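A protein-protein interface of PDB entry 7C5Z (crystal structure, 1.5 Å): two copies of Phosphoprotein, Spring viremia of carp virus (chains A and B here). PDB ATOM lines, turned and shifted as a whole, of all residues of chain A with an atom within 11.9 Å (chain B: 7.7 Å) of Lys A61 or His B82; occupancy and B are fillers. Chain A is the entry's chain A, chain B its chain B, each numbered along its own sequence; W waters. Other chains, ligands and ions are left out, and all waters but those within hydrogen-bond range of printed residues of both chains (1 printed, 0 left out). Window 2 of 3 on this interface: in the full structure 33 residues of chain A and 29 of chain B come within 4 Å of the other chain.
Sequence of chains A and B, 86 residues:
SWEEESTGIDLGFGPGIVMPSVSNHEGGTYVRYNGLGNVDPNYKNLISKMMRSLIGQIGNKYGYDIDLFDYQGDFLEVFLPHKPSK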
ATOM      1  N   ARG A  52       2.172  -5.546   0.550  1.00  0.00           N
ATOM      2  CA  ARG A  52       1.642  -5.381  -0.798  1.00  0.00           C
ATOM      3  C   ARG A  52       2.692  -5.725  -1.851  1.00  0.00           C
ATOM      4  O   ARG A  52       2.384  -6.393  -2.853  1.00  0.00           O
ATOM      5  CB  ARG A  52       1.114  -3.956  -0.976  1.00  0.00           C
ATOM      6  CG  ARG A  52       0.338  -3.760  -2.259  1.00  0.00           C
ATOM      7  CD  ARG A  52      -0.114  -2.318  -2.414  1.00  0.00           C
ATOM      8  NE  ARG A  52      -0.970  -1.843  -1.327  1.00  0.00           N
ATOM      9  CZ  ARG A  52      -2.276  -2.093  -1.230  1.00  0.00           C
ATOM     10  NH1 ARG A  52      -2.889  -2.843  -2.140  1.00  0.00           N
ATOM     11  NH2 ARG A  52      -2.973  -1.595  -0.214  1.00  0.00           N
ATOM     12  N   SER A  53       3.942  -5.315  -1.622  1.00  0.00           N
ATOM     13  CA  SER A  53       5.022  -5.630  -2.552  1.00  0.00           C
ATOM     14  C   SER A  53       5.258  -7.134  -2.609  1.00  0.00           C
ATOM     15  O   SER A  53       5.353  -7.727  -3.693  1.00  0.00           O
ATOM     16  CB  SER A  53       6.302  -4.894  -2.136  1.00  0.00           C
ATOM     17  OG  SER A  53       7.463  -5.525  -2.673  1.00  0.00           O
ATOM     18  N   LEU A  54       5.333  -7.774  -1.446  1.00  0.00           N
ATOM     19  CA  LEU A  54       5.629  -9.199  -1.407  1.00  0.00           C
ATOM     20  C   LEU A  54       4.520 -10.022  -2.052  1.00  0.00           C
ATOM     21  O   LEU A  54       4.801 -10.936  -2.833  1.00  0.00           O
ATOM     22  CB  LEU A  54       5.869  -9.648   0.034  1.00  0.00           C
ATOM     23  CG  LEU A  54       6.249 -11.111   0.199  1.00  0.00           C
ATOM     24  CD1 LEU A  54       7.475 -11.490  -0.626  1.00  0.00           C
ATOM     25  CD2 LEU A  54       6.503 -11.402   1.669  1.00  0.00           C
ATOM     26  N   ILE A  55       3.251  -9.738  -1.729  1.00  0.00           N
ATOM     27  CA  ILE A  55       2.183 -10.531  -2.348  1.00  0.00           C
ATOM     28  C   ILE A  55       2.119 -10.269  -3.851  1.00  0.00           C
ATOM     29  O   ILE A  55       1.665 -11.128  -4.616  1.00  0.00           O
ATOM     30  CB  ILE A  55       0.818 -10.282  -1.674  1.00  0.00           C
ATOM     31  CG1 ILE A  55       0.290  -8.885  -1.996  1.00  0.00           C
ATOM     32  CG2 ILE A  55       0.911 -10.505  -0.181  1.00  0.00           C
ATOM     33  CD1 ILE A  55      -1.077  -8.542  -1.336  1.00  0.00           C
ATOM     34  N   GLY A  56       2.551  -9.091  -4.302  1.00  0.00           N
ATOM     35  CA  GLY A  56       2.645  -8.856  -5.735  1.00  0.00           C
ATOM     36  C   GLY A  56       3.681  -9.751  -6.395  1.00  0.00           C
ATOM     37  O   GLY A  56       3.434 -10.320  -7.465  1.00  0.00           O
ATOM     38  N   GLN A  57       4.839  -9.904  -5.759  1.00  0.00           N
ATOM     39  CA  GLN A  57       5.877 -10.781  -6.284  1.00  0.00           C
ATOM     40  C   GLN A  57       5.428 -12.228  -6.254  1.00  0.00           C
ATOM     41  O   GLN A  57       5.656 -12.976  -7.210  1.00  0.00           O
ATOM     42  CB  GLN A  57       7.162 -10.611  -5.473  1.00  0.00           C
ATOM     43  CG  GLN A  57       7.767  -9.226  -5.572  1.00  0.00           C
ATOM     44  CD  GLN A  57       8.358  -8.940  -6.936  1.00  0.00           C
ATOM     45  OE1 GLN A  57       8.647  -9.858  -7.713  1.00  0.00           O
ATOM     46  NE2 GLN A  57       8.536  -7.660  -7.239  1.00  0.00           N
ATOM     47  N   ILE A  58       4.777 -12.640  -5.166  1.00  0.00           N
ATOM     48  CA  ILE A  58       4.339 -14.027  -5.043  1.00  0.00           C
ATOM     49  C   ILE A  58       3.216 -14.324  -6.031  1.00  0.00           C
ATOM     50  O   ILE A  58       3.220 -15.363  -6.705  1.00  0.00           O
ATOM     51  CB  ILE A  58       3.910 -14.322  -3.592  1.00  0.00           C
ATOM     52  CG1 ILE A  58       5.121 -14.285  -2.659  1.00  0.00           C
ATOM     53  CG2 ILE A  58       3.126 -15.660  -3.524  1.00  0.00           C
ATOM     54  CD1 ILE A  58       4.775 -14.332  -1.150  1.00  0.00           C
ATOM     55  N   GLY A  59       2.229 -13.432  -6.124  1.00  0.00           N
ATOM     56  CA  GLY A  59       1.128 -13.663  -7.052  1.00  0.00           C
ATOM     57  C   GLY A  59       1.585 -13.675  -8.499  1.00  0.00           C
ATOM     58  O   GLY A  59       1.081 -14.457  -9.315  1.00  0.00           O
ATOM     59  N   ASN A  60       2.559 -12.825  -8.834  1.00  0.00           N
ATOM     60  CA  ASN A  60       3.111 -12.833 -10.190  1.00  0.00           C
ATOM     61  C   ASN A  60       3.803 -14.154 -10.492  1.00  0.00           C
ATOM     62  O   ASN A  60       3.620 -14.731 -11.574  1.00  0.00           O
ATOM     63  CB  ASN A  60       4.108 -11.688 -10.369  1.00  0.00           C
ATOM     64  CG  ASN A  60       3.445 -10.350 -10.630  1.00  0.00           C
ATOM     65  OD1 ASN A  60       2.225 -10.248 -10.722  1.00  0.00           O
ATOM     66  ND2 ASN A  60       4.261  -9.309 -10.760  1.00  0.00           N
ATOM     67  N   LYS A  61       4.609 -14.645  -9.554  1.00  0.00           N
ATOM     68  CA  LYS A  61       5.378 -15.860  -9.804  1.00  0.00           C
ATOM     69  C   LYS A  61       4.468 -17.071  -9.937  1.00  0.00           C
ATOM     70  O   LYS A  61       4.620 -17.871 -10.865  1.00  0.00           O
ATOM     71  CB  LYS A  61       6.396 -16.094  -8.695  1.00  0.00           C
ATOM     72  CG  LYS A  61       7.266 -17.318  -8.936  1.00  0.00           C
ATOM     73  CD  LYS A  61       8.294 -17.468  -7.828  1.00  0.00           C
ATOM     74  CE  LYS A  61       9.183 -18.693  -8.030  1.00  0.00           C
ATOM     75  NZ  LYS A  61       9.986 -18.565  -9.285  1.00  0.00           N
ATOM     76  N   TYR A  62       3.518 -17.230  -9.019  1.00  0.00           N
ATOM     77  CA  TYR A  62       2.745 -18.461  -8.946  1.00  0.00           C
ATOM     78  C   TYR A  62       1.408 -18.382  -9.677  1.00  0.00           C
ATOM     79  O   TYR A  62       0.733 -19.412  -9.811  1.00  0.00           O
ATOM     80  CB  TYR A  62       2.534 -18.837  -7.477  1.00  0.00           C
ATOM     81  CG  TYR A  62       3.822 -19.158  -6.736  1.00  0.00           C
ATOM     82  CD1 TYR A  62       4.792 -19.989  -7.295  1.00  0.00           C
ATOM     83  CD2 TYR A  62       4.070 -18.637  -5.470  1.00  0.00           C
ATOM     84  CE1 TYR A  62       5.961 -20.289  -6.609  1.00  0.00           C
ATOM     85  CE2 TYR A  62       5.237 -18.934  -4.779  1.00  0.00           C
ATOM     86  CZ  TYR A  62       6.189 -19.754  -5.354  1.00  0.00           C
ATOM     87  OH  TYR A  62       7.332 -20.053  -4.655  1.00  0.00           O
ATOM     88  N   GLY A  63       1.011 -17.203 -10.144  1.00  0.00           N
ATOM     89  CA  GLY A  63      -0.173 -17.063 -10.971  1.00  0.00           C
ATOM     90  C   GLY A  63      -1.489 -16.965 -10.231  1.00  0.00           C
ATOM     91  O   GLY A  63      -2.499 -17.517 -10.694  1.00  0.00           O
ATOM     92  N   TYR A  64      -1.516 -16.256  -9.097  1.00  0.00           N
ATOM     93  CA  TYR A  64      -2.724 -15.999  -8.328  1.00  0.00           C
ATOM     94  C   TYR A  64      -2.851 -14.504  -8.091  1.00  0.00           C
ATOM     95  O   TYR A  64      -1.847 -13.830  -7.833  1.00  0.00           O
ATOM     96  CB  TYR A  64      -2.683 -16.720  -6.972  1.00  0.00           C
ATOM     97  CG  TYR A  64      -2.773 -18.214  -7.103  1.00  0.00           C
ATOM     98  CD1 TYR A  64      -4.006 -18.844  -7.195  1.00  0.00           C
ATOM     99  CD2 TYR A  64      -1.623 -18.990  -7.160  1.00  0.00           C
ATOM    100  CE1 TYR A  64      -4.097 -20.220  -7.334  1.00  0.00           C
ATOM    101  CE2 TYR A  64      -1.706 -20.374  -7.307  1.00  0.00           C
ATOM    102  CZ  TYR A  64      -2.945 -20.971  -7.382  1.00  0.00           C
ATOM    103  OH  TYR A  64      -3.029 -22.337  -7.516  1.00  0.00           O
ATOM    104  N   ASP A  65      -4.080 -13.999  -8.166  1.00  0.00           N
ATOM    105  CA  ASP A  65      -4.355 -12.573  -7.941  1.00  0.00           C
ATOM    106  C   ASP A  65      -4.539 -12.305  -6.445  1.00  0.00           C
ATOM    107  O   ASP A  65      -5.623 -11.983  -5.960  1.00  0.00           O
ATOM    108  CB  ASP A  65      -5.582 -12.136  -8.734  1.00  0.00           C
ATOM    109  CG  ASP A  65      -5.353 -12.176 -10.236  1.00  0.00           C
ATOM    110  OD1 ASP A  65      -4.202 -11.947 -10.667  1.00  0.00           O
ATOM    111  OD2 ASP A  65      -6.326 -12.443 -10.976  1.00  0.00           O
ATOM    112  N   ILE A  66      -3.449 -12.481  -5.699  1.00  0.00           N
ATOM    113  CA  ILE A  66      -3.457 -12.172  -4.269  1.00  0.00           C
ATOM    114  C   ILE A  66      -3.584 -10.668  -4.079  1.00  0.00           C
ATOM    115  O   ILE A  66      -2.948  -9.887  -4.799  1.00  0.00           O
ATOM    116  CB  ILE A  66      -2.178 -12.715  -3.609  1.00  0.00           C
ATOM    117  CG1 ILE A  66      -2.032 -14.219  -3.880  1.00  0.00           C
ATOM    118  CG2 ILE A  66      -2.163 -12.434  -2.096  1.00  0.00           C
ATOM    119  CD1 ILE A  66      -0.672 -14.763  -3.489  1.00  0.00           C
ATOM    120  N   PRO A  81      -6.999 -16.026  -3.584  1.00  0.00           N
ATOM    121  CA  PRO A  81      -8.042 -16.668  -4.399  1.00  0.00           C
ATOM    122  C   PRO A  81      -7.869 -18.180  -4.476  1.00  0.00           C
ATOM    123  O   PRO A  81      -6.750 -18.702  -4.478  1.00  0.00           O
ATOM    124  CB  PRO A  81      -7.876 -16.018  -5.781  1.00  0.00           C
ATOM    125  CG  PRO A  81      -6.503 -15.417  -5.787  1.00  0.00           C
ATOM    126  CD  PRO A  81      -6.125 -15.123  -4.354  1.00  0.00           C
ATOM    127  N   LYS A  83      -8.662 -19.994  -7.077  1.00  0.00           N
ATOM    128  CA  LYS A  83      -8.282 -20.410  -8.423  1.00  0.00           C
ATOM    129  C   LYS A  83      -7.243 -19.468  -9.020  1.00  0.00           C
ATOM    130  O   LYS A  83      -7.166 -18.299  -8.635  1.00  0.00           O
ATOM    131  CB  LYS A  83      -9.511 -20.464  -9.339  1.00  0.00           C
ATOM    132  CG  LYS A  83     -10.684 -21.199  -8.713  1.00  0.00           C
ATOM    133  CD  LYS A  83     -11.919 -21.139  -9.584  1.00  0.00           C
ATOM    134  CE  LYS A  83     -12.539 -22.516  -9.732  1.00  0.00           C
ATOM    135  NZ  LYS A  83     -14.005 -22.427  -9.960  1.00  0.00           N
ATOM    136  N   PRO A  84      -6.430 -19.945  -9.960  1.00  0.00           N
ATOM    137  CA  PRO A  84      -5.395 -19.093 -10.555  1.00  0.00           C
ATOM    138  C   PRO A  84      -5.999 -18.008 -11.432  1.00  0.00           C
ATOM    139  O   PRO A  84      -7.183 -18.021 -11.783  1.00  0.00           O
ATOM    140  CB  PRO A  84      -4.553 -20.069 -11.385  1.00  0.00           C
ATOM    141  CG  PRO A  84      -4.924 -21.437 -10.885  1.00  0.00           C
ATOM    142  CD  PRO A  84      -6.345 -21.331 -10.449  1.00  0.00           C
ATOM    143  N   SER A  85      -5.149 -17.058 -11.808  1.00  0.00           N
ATOM    144  CA  SER A  85      -5.606 -15.923 -12.609  1.00  0.00           C
ATOM    145  C   SER A  85      -6.054 -16.378 -13.993  1.00  0.00           C
ATOM    146  O   SER A  85      -5.480 -17.310 -14.548  1.00  0.00           O
ATOM    147  CB  SER A  85      -4.501 -14.875 -12.735  1.00  0.00           C
ATOM    148  OG  SER A  85      -3.749 -14.805 -11.540  1.00  0.00           O
ATOM    149  N   VAL B  22      14.888  -8.503  -6.692  1.00  0.00           N
ATOM    150  CA  VAL B  22      14.408  -9.844  -6.996  1.00  0.00           C
ATOM    151  C   VAL B  22      15.451 -10.543  -7.852  1.00  0.00           C
ATOM    152  O   VAL B  22      15.865  -9.999  -8.880  1.00  0.00           O
ATOM    153  CB  VAL B  22      13.057  -9.788  -7.726  1.00  0.00           C
ATOM    154  CG1 VAL B  22      12.547 -11.177  -7.987  1.00  0.00           C
ATOM    155  CG2 VAL B  22      12.029  -8.970  -6.903  1.00  0.00           C
ATOM    156  N   SER B  23      15.871 -11.744  -7.439  1.00  0.00           N
ATOM    157  CA  SER B  23      16.898 -12.478  -8.183  1.00  0.00           C
ATOM    158  C   SER B  23      16.512 -13.940  -8.355  1.00  0.00           C
ATOM    159  O   SER B  23      15.855 -14.535  -7.497  1.00  0.00           O
ATOM    160  CB  SER B  23      18.278 -12.364  -7.504  1.00  0.00           C
ATOM    161  OG  SER B  23      18.272 -12.851  -6.175  1.00  0.00           O
ATOM    162  N   ASN B  24      16.945 -14.509  -9.480  1.00  0.00           N
ATOM    163  CA  ASN B  24      16.569 -15.846  -9.917  1.00  0.00           C
ATOM    164  C   ASN B  24      17.723 -16.799  -9.657  1.00  0.00           C
ATOM    165  O   ASN B  24      18.840 -16.569 -10.132  1.00  0.00           O
ATOM    166  CB  ASN B  24      16.226 -15.840 -11.406  1.00  0.00           C
ATOM    167  CG  ASN B  24      15.867 -17.216 -11.924  1.00  0.00           C
ATOM    168  OD1 ASN B  24      16.669 -17.886 -12.584  1.00  0.00           O
ATOM    169  ND2 ASN B  24      14.661 -17.653 -11.615  1.00  0.00           N
ATOM    170  N   HIS B  25      17.455 -17.867  -8.927  1.00  0.00           N
ATOM    171  CA  HIS B  25      18.478 -18.843  -8.599  1.00  0.00           C
ATOM    172  C   HIS B  25      18.011 -20.212  -9.081  1.00  0.00           C
ATOM    173  O   HIS B  25      16.918 -20.356  -9.618  1.00  0.00           O
ATOM    174  CB  HIS B  25      18.771 -18.816  -7.100  1.00  0.00           C
ATOM    175  CG  HIS B  25      19.287 -17.494  -6.619  1.00  0.00           C
ATOM    176  ND1 HIS B  25      20.543 -17.337  -6.077  1.00  0.00           N
ATOM    177  CD2 HIS B  25      18.725 -16.259  -6.626  1.00  0.00           C
ATOM    178  CE1 HIS B  25      20.730 -16.068  -5.755  1.00  0.00           C
ATOM    179  NE2 HIS B  25      19.641 -15.393  -6.078  1.00  0.00           N
ATOM    180  N   GLU B  26      18.873 -21.220  -8.910  1.00  0.00           N
ATOM    181  CA  GLU B  26      18.566 -22.534  -9.467  1.00  0.00           C
ATOM    182  C   GLU B  26      17.287 -23.111  -8.870  1.00  0.00           C
ATOM    183  O   GLU B  26      16.472 -23.694  -9.593  1.00  0.00           O
ATOM    184  CB  GLU B  26      19.737 -23.492  -9.255  1.00  0.00           C
ATOM    185  CG  GLU B  26      19.501 -24.866  -9.862  1.00  0.00           C
ATOM    186  CD  GLU B  26      20.789 -25.578 -10.223  1.00  0.00           C
ATOM    187  OE1 GLU B  26      21.673 -25.694  -9.348  1.00  0.00           O
ATOM    188  OE2 GLU B  26      20.916 -26.018 -11.387  1.00  0.00           O
ATOM    189  N   GLY B  27      17.077 -22.924  -7.565  1.00  0.00           N
ATOM    190  CA  GLY B  27      15.946 -23.529  -6.880  1.00  0.00           C
ATOM    191  C   GLY B  27      14.747 -22.631  -6.639  1.00  0.00           C
ATOM    192  O   GLY B  27      13.664 -23.117  -6.291  1.00  0.00           O
ATOM    193  N   GLY B  28      14.910 -21.328  -6.825  1.00  0.00           N
ATOM    194  CA  GLY B  28      13.796 -20.428  -6.593  1.00  0.00           C
ATOM    195  C   GLY B  28      14.213 -18.987  -6.767  1.00  0.00           C
ATOM    196  O   GLY B  28      15.290 -18.690  -7.286  1.00  0.00           O
ATOM    197  N   THR B  29      13.331 -18.097  -6.316  1.00  0.00           N
ATOM    198  CA  THR B  29      13.471 -16.654  -6.464  1.00  0.00           C
ATOM    199  C   THR B  29      13.677 -16.048  -5.084  1.00  0.00           C
ATOM    200  O   THR B  29      12.957 -16.401  -4.142  1.00  0.00           O
ATOM    201  CB  THR B  29      12.217 -16.063  -7.109  1.00  0.00           C
ATOM    202  OG1 THR B  29      12.035 -16.618  -8.423  1.00  0.00           O
ATOM    203  CG2 THR B  29      12.293 -14.548  -7.188  1.00  0.00           C
ATOM    204  N   TYR B  30      14.645 -15.150  -4.961  1.00  0.00           N
ATOM    205  CA  TYR B  30      14.867 -14.417  -3.722  1.00  0.00           C
ATOM    206  C   TYR B  30      14.331 -13.004  -3.886  1.00  0.00           C
ATOM    207  O   TYR B  30      14.604 -12.343  -4.894  1.00  0.00           O
ATOM    208  CB  TYR B  30      16.351 -14.388  -3.335  1.00  0.00           C
ATOM    209  CG  TYR B  30      16.844 -15.690  -2.740  1.00  0.00           C
ATOM    210  CD1 TYR B  30      17.368 -16.680  -3.553  1.00  0.00           C
ATOM    211  CD2 TYR B  30      16.784 -15.927  -1.371  1.00  0.00           C
ATOM    212  CE1 TYR B  30      17.823 -17.877  -3.031  1.00  0.00           C
ATOM    213  CE2 TYR B  30      17.238 -17.126  -0.835  1.00  0.00           C
ATOM    214  CZ  TYR B  30      17.757 -18.093  -1.674  1.00  0.00           C
ATOM    215  OH  TYR B  30      18.212 -19.290  -1.164  1.00  0.00           O
ATOM    216  N   VAL B  31      13.543 -12.561  -2.905  1.00  0.00           N
ATOM    217  CA  VAL B  31      13.020 -11.199  -2.830  1.00  0.00           C
ATOM    218  C   VAL B  31      13.628 -10.551  -1.593  1.00  0.00           C
ATOM    219  O   VAL B  31      13.322 -10.950  -0.462  1.00  0.00           O
ATOM    220  CB  VAL B  31      11.492 -11.173  -2.742  1.00  0.00           C
ATOM    221  CG1 VAL B  31      11.013  -9.735  -2.832  1.00  0.00           C
ATOM    222  CG2 VAL B  31      10.876 -12.017  -3.841  1.00  0.00           C
ATOM    223  N   TYR B  64       3.544 -24.267  -1.435  1.00  0.00           N
ATOM    224  CA  TYR B  64       4.936 -23.931  -1.693  1.00  0.00           C
ATOM    225  C   TYR B  64       5.632 -23.663  -0.370  1.00  0.00           C
ATOM    226  O   TYR B  64       5.065 -23.016   0.520  1.00  0.00           O
ATOM    227  CB  TYR B  64       5.065 -22.698  -2.587  1.00  0.00           C
ATOM    228  CG  TYR B  64       4.613 -22.906  -4.011  1.00  0.00           C
ATOM    229  CD1 TYR B  64       5.504 -23.340  -4.984  1.00  0.00           C
ATOM    230  CD2 TYR B  64       3.296 -22.674  -4.382  1.00  0.00           C
ATOM    231  CE1 TYR B  64       5.094 -23.531  -6.291  1.00  0.00           C
ATOM    232  CE2 TYR B  64       2.875 -22.863  -5.679  1.00  0.00           C
ATOM    233  CZ  TYR B  64       3.777 -23.293  -6.633  1.00  0.00           C
ATOM    234  OH  TYR B  64       3.362 -23.476  -7.929  1.00  0.00           O
ATOM    235  N   PHE B  79      12.428 -16.442   0.198  1.00  0.00           N
ATOM    236  CA  PHE B  79      12.718 -17.441  -0.828  1.00  0.00           C
ATOM    237  C   PHE B  79      11.419 -18.053  -1.348  1.00  0.00           C
ATOM    238  O   PHE B  79      10.659 -18.644  -0.574  1.00  0.00           O
ATOM    239  CB  PHE B  79      13.613 -18.548  -0.269  1.00  0.00           C
ATOM    240  CG  PHE B  79      13.918 -19.643  -1.265  1.00  0.00           C
ATOM    241  CD1 PHE B  79      14.738 -19.390  -2.363  1.00  0.00           C
ATOM    242  CD2 PHE B  79      13.399 -20.918  -1.101  1.00  0.00           C
ATOM    243  CE1 PHE B  79      15.036 -20.397  -3.291  1.00  0.00           C
ATOM    244  CE2 PHE B  79      13.693 -21.931  -2.028  1.00  0.00           C
ATOM    245  CZ  PHE B  79      14.507 -21.660  -3.119  1.00  0.00           C
ATOM    246  N   LEU B  80      11.177 -17.922  -2.653  1.00  0.00           N
ATOM    247  CA  LEU B  80      10.028 -18.505  -3.344  1.00  0.00           C
ATOM    248  C   LEU B  80      10.500 -19.692  -4.172  1.00  0.00           C
ATOM    249  O   LEU B  80      11.099 -19.500  -5.244  1.00  0.00           O
ATOM    250  CB  LEU B  80       9.353 -17.469  -4.249  1.00  0.00           C
ATOM    251  CG  LEU B  80       9.083 -16.106  -3.602  1.00  0.00           C
ATOM    252  CD1 LEU B  80       8.425 -15.176  -4.613  1.00  0.00           C
ATOM    253  CD2 LEU B  80       8.223 -16.257  -2.364  1.00  0.00           C
ATOM    254  N   PRO B  81      10.268 -20.925  -3.733  1.00  0.00           N
ATOM    255  CA  PRO B  81      10.693 -22.081  -4.539  1.00  0.00           C
ATOM    256  C   PRO B  81      10.028 -22.084  -5.906  1.00  0.00           C
ATOM    257  O   PRO B  81       8.881 -21.664  -6.074  1.00  0.00           O
ATOM    258  CB  PRO B  81      10.233 -23.291  -3.716  1.00  0.00           C
ATOM    259  CG  PRO B  81       9.846 -22.768  -2.380  1.00  0.00           C
ATOM    260  CD  PRO B  81       9.498 -21.320  -2.542  1.00  0.00           C
ATOM    261  N   HIS B  82      10.759 -22.583  -6.905  1.00  0.00           N
ATOM    262  CA  HIS B  82      10.178 -22.686  -8.236  1.00  0.00           C
ATOM    263  C   HIS B  82       9.068 -23.727  -8.285  1.00  0.00           C
ATOM    264  O   HIS B  82       8.091 -23.553  -9.017  1.00  0.00           O
ATOM    265  CB  HIS B  82      11.252 -23.053  -9.269  1.00  0.00           C
ATOM    266  CG  HIS B  82      12.263 -21.974  -9.532  1.00  0.00           C
ATOM    267  ND1 HIS B  82      11.928 -20.643  -9.663  1.00  0.00           N
ATOM    268  CD2 HIS B  82      13.604 -22.040  -9.714  1.00  0.00           C
ATOM    269  CE1 HIS B  82      13.019 -19.935  -9.901  1.00  0.00           C
ATOM    270  NE2 HIS B  82      14.050 -20.759  -9.939  1.00  0.00           N
ATOM    271  N   LYS B  83       9.209 -24.806  -7.519  1.00  0.00           N
ATOM    272  CA  LYS B  83       8.359 -25.986  -7.564  1.00  0.00           C
ATOM    273  C   LYS B  83       7.564 -26.134  -6.273  1.00  0.00           C
ATOM    274  O   LYS B  83       8.058 -25.788  -5.194  1.00  0.00           O
ATOM    275  CB  LYS B  83       9.203 -27.250  -7.774  1.00  0.00           C
ATOM    276  CG  LYS B  83       9.723 -27.427  -9.194  1.00  0.00           C
ATOM    277  CD  LYS B  83       8.761 -26.845 -10.213  1.00  0.00           C
ATOM    278  CE  LYS B  83       9.490 -26.404 -11.473  1.00  0.00           C
ATOM    279  NZ  LYS B  83       8.592 -26.451 -12.660  1.00  0.00           N
ATOM    280  N   PRO B  84       6.340 -26.652  -6.353  1.00  0.00           N
ATOM    281  CA  PRO B  84       5.576 -26.946  -5.137  1.00  0.00           C
ATOM    282  C   PRO B  84       6.226 -28.064  -4.340  1.00  0.00           C
ATOM    283  O   PRO B  84       7.028 -28.847  -4.851  1.00  0.00           O
ATOM    284  CB  PRO B  84       4.199 -27.370  -5.666  1.00  0.00           C
ATOM    285  CG  PRO B  84       4.420 -27.740  -7.097  1.00  0.00           C
ATOM    286  CD  PRO B  84       5.567 -26.906  -7.581  1.00  0.00           C
ATOM    287  N   SER B  85       5.866 -28.125  -3.057  1.00  0.00           N
ATOM    288  CA  SER B  85       6.493 -29.093  -2.163  1.00  0.00           C
ATOM    289  C   SER B  85       6.144 -30.526  -2.545  1.00  0.00           C
ATOM    290  O   SER B  85       6.961 -31.432  -2.354  1.00  0.00           O
ATOM    291  CB  SER B  85       6.087 -28.813  -0.718  1.00  0.00           C
ATOM    292  OG  SER B  85       4.687 -28.659  -0.604  1.00  0.00           O
HETATM  293  O   HOH W   1       1.509 -21.943  -9.125  1.00  0.00           O
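NZ of Lys A61 lies within hydrogen-bond range of OG1 of Thr B29 (3.0 Å). NZ of Lys A61 is in hydrogen-bond range of ND1 of His B82, at 2.9 Å. The backbone carbonyl oxygen of Pro B81 sits at hydrogen-bond distance from the side-chain hydroxyl of Tyr A62 (2.6 Å).
The backbone carbonyl oxygen (O) of His B25 lies within hydrogen-bond range of a ring nitrogen (NE2) of His B82, 2.9 Å away. The backbone carbonyl oxygen (O) of Gly B27 is in hydrogen-bond range of the backbone NH (N) of His B82, 3.0 Å away. The backbone NH (N) of Gly B28 lies close to a ring nitrogen (NE2) of His B82, at 3.3 Å. The backbone NH of Leu B80 lies within hydrogen-bond range of the backbone carbonyl oxygen of Thr B29.
Among the printed residues, merely in contact across the chains: Tyr A62 with Leu B80, Tyr A62 with Tyr B64, Lys A61 with Leu B80, Lys A61 with Pro B81, Gln A57 with Val B22 and Ile A58 with Leu B80.
Lys A61 touches just these residues of chain B: Thr B29, Leu B80, Pro B81 and His B82. His B82 touches one residue of chain A. No residue of chain A comes within 4 Å of Asn B24. No residue of chain A comes within 4 Å of Gly B27. Thr B29 touches just one residue of chain A: Lys A61. Of chain A, only Ile A58, Lys A61 and Tyr A62 come within 4 Å of Leu B80. Pro B81 touches two residues of chain A. No residue of chain A comes within 4 Å of Lys B83. Of the printed residues of chain A, Tyr B64 touches Tyr A62. Of the printed residues of chain B, Tyr A62 touches Tyr B64 (3.4 Å), Leu B80 (3.2 Å) and Pro B81 (2.6 Å). Of the printed residues of chain B, Ile A58 touches Leu B80. Of the printed residues of chain B, Gln A57 touches Val B22. Of the printed residues of chain A, Val B22 touches Gln A57. Ser B85 touches none of the printed residues of chain A. Pro A81 touches none of the printed residues of chain B. The nearest residue of chain A that does not touch His B82 is Tyr A62 (4.6 Å).
Of the 19 printed residues of chain A, 4 touch a printed residue of chain B. Hydrophobic or aromatic side chains of chain A that line the printed part of chain B: Ile A58 and Tyr A62. Of the 18 printed residues of chain B, 6 touch a printed residue of chain A. Hydrophobic or aromatic side chains of chain B within 4 Å of the printed part of chain A: Val B22, Tyr B64, Leu B80, Pro B81 and His B82.
Positions printed for both chains: 64, 81, 83, 84 and 85. Of the 9 pairs that touch across the chains among the printed residues, none has its exchanged pair printed and touching as well.
Water W1 bridges the side-chain hydroxyl (OH) of Tyr B64 (2.7 Å) and the backbone carbonyl oxygen (O) of Tyr A62 (2.7 Å).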
